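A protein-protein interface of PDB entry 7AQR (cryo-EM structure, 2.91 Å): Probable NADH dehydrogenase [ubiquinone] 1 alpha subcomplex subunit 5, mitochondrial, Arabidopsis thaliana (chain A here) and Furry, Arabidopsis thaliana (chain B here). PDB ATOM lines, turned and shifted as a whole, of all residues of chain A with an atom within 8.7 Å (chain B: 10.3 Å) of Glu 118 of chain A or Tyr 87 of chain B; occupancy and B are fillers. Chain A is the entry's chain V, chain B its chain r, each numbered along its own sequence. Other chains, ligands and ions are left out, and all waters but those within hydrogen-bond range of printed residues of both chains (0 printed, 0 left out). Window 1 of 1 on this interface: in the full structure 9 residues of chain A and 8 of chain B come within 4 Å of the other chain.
O of Arg 85 of chain B sits close to O of Val 119 of chain A (2.9 Å). N of Glu 121 of chain A lies within hydrogen-bond range of O of Arg 85 of chain B (3.4 Å). The backbone carbonyl oxygen of Cys 117 of chain A lies within hydrogen-bond range of the backbone NH of Leu 89 of chain B (2.6 Å). The backbone carbonyl oxygen (O) of Tyr 87 of chain B lies within hydrogen-bond range of the backbone NH (N) of Val 119 of chain A (3.0 Å).
Of the printed residues of chain B, Glu 116 of chain A touches Val 88 and Leu 89. Of the printed residues of chain B, Glu 118 of chain A touches Tyr 87 (3.8 Å) and Val 88 (3.96 Å). Of the printed residues of chain B, Asn 122 of chain A touches Ile 84. Of the printed residues of chain A, Ile 84 of chain B touches Ile 120, Glu 121 and Asn 122. Printed residues of chain A within 4 Å of Tyr 87 of chain B: Cys 117 (3.9 Å), Glu 118 (3.8 Å) and Val 119 (3.0 Å). Val 88 of chain B touches three residues of chain A. Of the printed residues of chain A, Leu 89 of chain B touches Tyr 115 (3.8 Å), Glu 116 (3.3 Å), Cys 117 (2.6 Å) and Val 119 (3.6 Å). Asp 92 of chain B touches none of the printed residues of chain A. The nearest residue of chain B that does not touch Glu 118 of chain A is Leu 89 of chain B (4.8 Å). The nearest residue of chain A that does not touch Tyr 87 of chain B is Glu 121 of chain A (4.1 Å). The nearest printed residue of chain A that does not touch Arg 86 of chain B is Val 119 of chain A (4.03 Å).
Among the printed residues, merely in contact across the chains: Cys 117 of chain A with Val 88 of chain B, Glu 116 of chain A with Leu 89 of chain B, Glu 121 of chain A with Ile 84 of chain B, Asn 122 of chain A with Ile 84 of chain B, Val 119 of chain A with Leu 89 of chain B, Glu 116 of chain A with Val 88 of chain B, Ile 120 of chain A with Ile 84 of chain B, Glu 118 of chain A with Tyr 87 of chain B, Tyr 115 of chain A with Thr 90 of chain B, Tyr 115 of chain A with Leu 89 of chain B, Ile 120 of chain A with Arg 85 of chain B, Cys 117 of chain A with Tyr 87 of chain B, Ile 120 of chain A with Arg 86 of chain B and Glu 118 of chain A with Val 88 of chain B.
Hydrophobic or aromatic side chains of chain A that line the printed part of chain B: Tyr 115, Val 119 and Ile 120. Along chain A the printed residues that touch a printed residue of chain B span positions 115 to 122. Of the 8 printed residues of chain B, 7 touch a printed residue of chain A. Printed residues of chain B that touch a printed residue of chain A: Ile 84, Arg 85, Arg 86, Tyr 87, Val 88, Leu 89 and Thr 90. Hydrophobic or aromatic side chains of chain B that line the printed part of chain A: Ile 84, Tyr 87, Val 88 and Leu 89. Among the printed residues, 18 pairs touch across the chains.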
ATOM      1  N   TYR A 115      27.724   6.201  39.495  1.00  0.00           N
ATOM      2  CA  TYR A 115      28.419   7.024  38.515  1.00  0.00           C
ATOM      3  C   TYR A 115      27.459   7.547  37.455  1.00  0.00           C
ATOM      4  O   TYR A 115      26.561   6.836  36.998  1.00  0.00           O
ATOM      5  CB  TYR A 115      29.541   6.216  37.860  1.00  0.00           C
ATOM      6  CG  TYR A 115      30.021   6.782  36.543  1.00  0.00           C
ATOM      7  CD1 TYR A 115      30.918   7.840  36.503  1.00  0.00           C
ATOM      8  CD2 TYR A 115      29.584   6.249  35.337  1.00  0.00           C
ATOM      9  CE1 TYR A 115      31.357   8.357  35.302  1.00  0.00           C
ATOM     10  CE2 TYR A 115      30.018   6.759  34.132  1.00  0.00           C
ATOM     11  CZ  TYR A 115      30.905   7.812  34.119  1.00  0.00           C
ATOM     12  OH  TYR A 115      31.341   8.321  32.918  1.00  0.00           O
ATOM     13  N   GLU A 116      27.660   8.805  37.064  1.00  0.00           N
ATOM     14  CA  GLU A 116      26.887   9.426  35.998  1.00  0.00           C
ATOM     15  C   GLU A 116      27.717  10.546  35.390  1.00  0.00           C
ATOM     16  O   GLU A 116      28.401  11.275  36.115  1.00  0.00           O
ATOM     17  CB  GLU A 116      25.546   9.958  36.519  1.00  0.00           C
ATOM     18  CG  GLU A 116      25.658  10.991  37.630  1.00  0.00           C
ATOM     19  CD  GLU A 116      25.684  12.413  37.106  1.00  0.00           C
ATOM     20  OE1 GLU A 116      25.206  12.637  35.974  1.00  0.00           O
ATOM     21  OE2 GLU A 116      26.183  13.306  37.821  1.00  0.00           O
ATOM     22  N   CYS A 117      27.667  10.673  34.066  1.00  0.00           N
ATOM     23  CA  CYS A 117      28.448  11.670  33.342  1.00  0.00           C
ATOM     24  C   CYS A 117      27.566  12.332  32.296  1.00  0.00           C
ATOM     25  O   CYS A 117      26.905  11.643  31.513  1.00  0.00           O
ATOM     26  CB  CYS A 117      29.676  11.034  32.684  1.00  0.00           C
ATOM     27  SG  CYS A 117      30.783  12.200  31.861  1.00  0.00           S
ATOM     28  N   GLU A 118      27.561  13.664  32.280  1.00  0.00           N
ATOM     29  CA  GLU A 118      26.811  14.432  31.287  1.00  0.00           C
ATOM     30  C   GLU A 118      27.733  14.727  30.113  1.00  0.00           C
ATOM     31  O   GLU A 118      28.619  15.579  30.187  1.00  0.00           O
ATOM     32  CB  GLU A 118      26.255  15.715  31.896  1.00  0.00           C
ATOM     33  CG  GLU A 118      25.369  15.516  33.118  1.00  0.00           C
ATOM     34  CD  GLU A 118      26.154  15.405  34.411  1.00  0.00           C
ATOM     35  OE1 GLU A 118      25.865  16.178  35.348  1.00  0.00           O
ATOM     36  OE2 GLU A 118      27.051  14.541  34.496  1.00  0.00           O
ATOM     37  N   VAL A 119      27.523  14.012  29.010  1.00  0.00           N
ATOM     38  CA  VAL A 119      28.326  14.197  27.808  1.00  0.00           C
ATOM     39  C   VAL A 119      27.651  15.206  26.889  1.00  0.00           C
ATOM     40  O   VAL A 119      26.849  14.836  26.025  1.00  0.00           O
ATOM     41  CB  VAL A 119      28.556  12.861  27.080  1.00  0.00           C
ATOM     42  CG1 VAL A 119      29.505  13.051  25.910  1.00  0.00           C
ATOM     43  CG2 VAL A 119      29.104  11.834  28.044  1.00  0.00           C
ATOM     44  N   ILE A 120      27.966  16.484  27.074  1.00  0.00           N
ATOM     45  CA  ILE A 120      27.448  17.543  26.215  1.00  0.00           C
ATOM     46  C   ILE A 120      28.134  17.460  24.859  1.00  0.00           C
ATOM     47  O   ILE A 120      29.345  17.234  24.775  1.00  0.00           O
ATOM     48  CB  ILE A 120      27.636  18.931  26.858  1.00  0.00           C
ATOM     49  CG1 ILE A 120      26.842  19.039  28.162  1.00  0.00           C
ATOM     50  CG2 ILE A 120      27.231  20.036  25.898  1.00  0.00           C
ATOM     51  CD1 ILE A 120      27.590  18.587  29.387  1.00  0.00           C
ATOM     52  N   GLU A 121      27.361  17.634  23.786  1.00  0.00           N
ATOM     53  CA  GLU A 121      27.918  17.602  22.436  1.00  0.00           C
ATOM     54  C   GLU A 121      27.416  18.851  21.712  1.00  0.00           C
ATOM     55  O   GLU A 121      26.306  18.850  21.175  1.00  0.00           O
ATOM     56  CB  GLU A 121      27.517  16.332  21.703  1.00  0.00           C
ATOM     57  CG  GLU A 121      28.191  15.075  22.225  1.00  0.00           C
ATOM     58  CD  GLU A 121      29.661  15.015  21.872  1.00  0.00           C
ATOM     59  OE1 GLU A 121      30.031  15.503  20.784  1.00  0.00           O
ATOM     60  OE2 GLU A 121      30.448  14.483  22.683  1.00  0.00           O
ATOM     61  N   ASN A 122      28.234  19.896  21.711  1.00  0.00           N
ATOM     62  CA  ASN A 122      27.893  21.134  21.031  1.00  0.00           C
ATOM     63  C   ASN A 122      28.427  21.117  19.602  1.00  0.00           C
ATOM     64  O   ASN A 122      29.457  20.510  19.302  1.00  0.00           O
ATOM     65  CB  ASN A 122      28.451  22.337  21.791  1.00  0.00           C
ATOM     66  CG  ASN A 122      27.891  23.652  21.291  1.00  0.00           C
ATOM     67  OD1 ASN A 122      26.701  23.930  21.437  1.00  0.00           O
ATOM     68  ND2 ASN A 122      28.750  24.471  20.696  1.00  0.00           N
ATOM     69  N   ILE B  84      20.892  20.949  22.907  1.00  0.00           N
ATOM     70  CA  ILE B  84      22.218  20.346  22.858  1.00  0.00           C
ATOM     71  C   ILE B  84      22.121  18.885  23.289  1.00  0.00           C
ATOM     72  O   ILE B  84      21.301  18.535  24.137  1.00  0.00           O
ATOM     73  CB  ILE B  84      23.215  21.125  23.734  1.00  0.00           C
ATOM     74  CG1 ILE B  84      23.086  22.627  23.476  1.00  0.00           C
ATOM     75  CG2 ILE B  84      24.638  20.680  23.448  1.00  0.00           C
ATOM     76  CD1 ILE B  84      23.371  23.030  22.046  1.00  0.00           C
ATOM     77  N   ARG B  85      22.964  18.036  22.703  1.00  0.00           N
ATOM     78  CA  ARG B  85      22.923  16.603  22.974  1.00  0.00           C
ATOM     79  C   ARG B  85      23.506  16.292  24.347  1.00  0.00           C
ATOM     80  O   ARG B  85      24.590  15.711  24.452  1.00  0.00           O
ATOM     81  CB  ARG B  85      23.676  15.840  21.883  1.00  0.00           C
ATOM     82  CG  ARG B  85      23.226  16.193  20.472  1.00  0.00           C
ATOM     83  CD  ARG B  85      24.160  15.624  19.417  1.00  0.00           C
ATOM     84  NE  ARG B  85      24.609  14.277  19.740  1.00  0.00           N
ATOM     85  CZ  ARG B  85      25.717  13.724  19.265  1.00  0.00           C
ATOM     86  NH1 ARG B  85      26.514  14.378  18.436  1.00  0.00           N
ATOM     87  NH2 ARG B  85      26.032  12.485  19.629  1.00  0.00           N
ATOM     88  N   ARG B  86      22.786  16.668  25.403  1.00  0.00           N
ATOM     89  CA  ARG B  86      23.265  16.508  26.776  1.00  0.00           C
ATOM     90  C   ARG B  86      22.766  15.195  27.382  1.00  0.00           C
ATOM     91  O   ARG B  86      22.134  15.163  28.437  1.00  0.00           O
ATOM     92  CB  ARG B  86      22.835  17.700  27.623  1.00  0.00           C
ATOM     93  CG  ARG B  86      22.978  19.044  26.934  1.00  0.00           C
ATOM     94  CD  ARG B  86      22.374  20.156  27.777  1.00  0.00           C
ATOM     95  NE  ARG B  86      23.351  20.761  28.675  1.00  0.00           N
ATOM     96  CZ  ARG B  86      23.462  20.471  29.964  1.00  0.00           C
ATOM     97  NH1 ARG B  86      22.672  19.582  30.544  1.00  0.00           N
ATOM     98  NH2 ARG B  86      24.389  21.089  30.690  1.00  0.00           N
ATOM     99  N   TYR B  87      23.059  14.095  26.693  1.00  0.00           N
ATOM    100  CA  TYR B  87      22.711  12.792  27.238  1.00  0.00           C
ATOM    101  C   TYR B  87      23.621  12.463  28.423  1.00  0.00           C
ATOM    102  O   TYR B  87      24.753  12.938  28.528  1.00  0.00           O
ATOM    103  CB  TYR B  87      22.793  11.714  26.157  1.00  0.00           C
ATOM    104  CG  TYR B  87      24.154  11.539  25.523  1.00  0.00           C
ATOM    105  CD1 TYR B  87      24.541  12.315  24.440  1.00  0.00           C
ATOM    106  CD2 TYR B  87      25.041  10.581  25.993  1.00  0.00           C
ATOM    107  CE1 TYR B  87      25.781  12.151  23.852  1.00  0.00           C
ATOM    108  CE2 TYR B  87      26.283  10.410  25.412  1.00  0.00           C
ATOM    109  CZ  TYR B  87      26.647  11.198  24.341  1.00  0.00           C
ATOM    110  OH  TYR B  87      27.881  11.033  23.758  1.00  0.00           O
ATOM    111  N   VAL B  88      23.103  11.637  29.329  1.00  0.00           N
ATOM    112  CA  VAL B  88      23.743  11.370  30.618  1.00  0.00           C
ATOM    113  C   VAL B  88      24.162   9.903  30.624  1.00  0.00           C
ATOM    114  O   VAL B  88      23.335   9.002  30.454  1.00  0.00           O
ATOM    115  CB  VAL B  88      22.831  11.691  31.805  1.00  0.00           C
ATOM    116  CG1 VAL B  88      23.506  11.304  33.110  1.00  0.00           C
ATOM    117  CG2 VAL B  88      22.466  13.166  31.807  1.00  0.00           C
ATOM    118  N   LEU B  89      25.456   9.655  30.822  1.00  0.00           N
ATOM    119  CA  LEU B  89      25.945   8.291  30.968  1.00  0.00           C
ATOM    120  C   LEU B  89      25.546   7.724  32.323  1.00  0.00           C
ATOM    121  O   LEU B  89      25.277   8.464  33.273  1.00  0.00           O
ATOM    122  CB  LEU B  89      27.466   8.247  30.817  1.00  0.00           C
ATOM    123  CG  LEU B  89      28.063   8.598  29.456  1.00  0.00           C
ATOM    124  CD1 LEU B  89      29.578   8.630  29.553  1.00  0.00           C
ATOM    125  CD2 LEU B  89      27.610   7.614  28.391  1.00  0.00           C
ATOM    126  N   THR B  90      25.540   6.400  32.415  1.00  0.00           N
ATOM    127  CA  THR B  90      25.197   5.711  33.652  1.00  0.00           C
ATOM    128  C   THR B  90      26.101   4.485  33.790  1.00  0.00           C
ATOM    129  O   THR B  90      26.868   4.169  32.881  1.00  0.00           O
ATOM    130  CB  THR B  90      23.713   5.291  33.674  1.00  0.00           C
ATOM    131  OG1 THR B  90      22.880   6.454  33.583  1.00  0.00           O
ATOM    132  CG2 THR B  90      23.379   4.539  34.959  1.00  0.00           C
ATOM    133  N   ASP B  92      25.244   1.351  33.812  1.00  0.00           N
ATOM    134  CA  ASP B  92      24.766   0.363  32.840  1.00  0.00           C
ATOM    135  C   ASP B  92      25.222  -1.064  33.151  1.00  0.00           C
ATOM    136  O   ASP B  92      25.585  -1.815  32.245  1.00  0.00           O
ATOM    137  CB  ASP B  92      25.142   0.756  31.404  1.00  0.00           C
ATOM    138  CG  ASP B  92      24.576   2.104  31.001  1.00  0.00           C
ATOM    139  OD1 ASP B  92      23.641   2.584  31.675  1.00  0.00           O
ATOM    140  OD2 ASP B  92      25.065   2.681  30.007  1.00  0.00           O
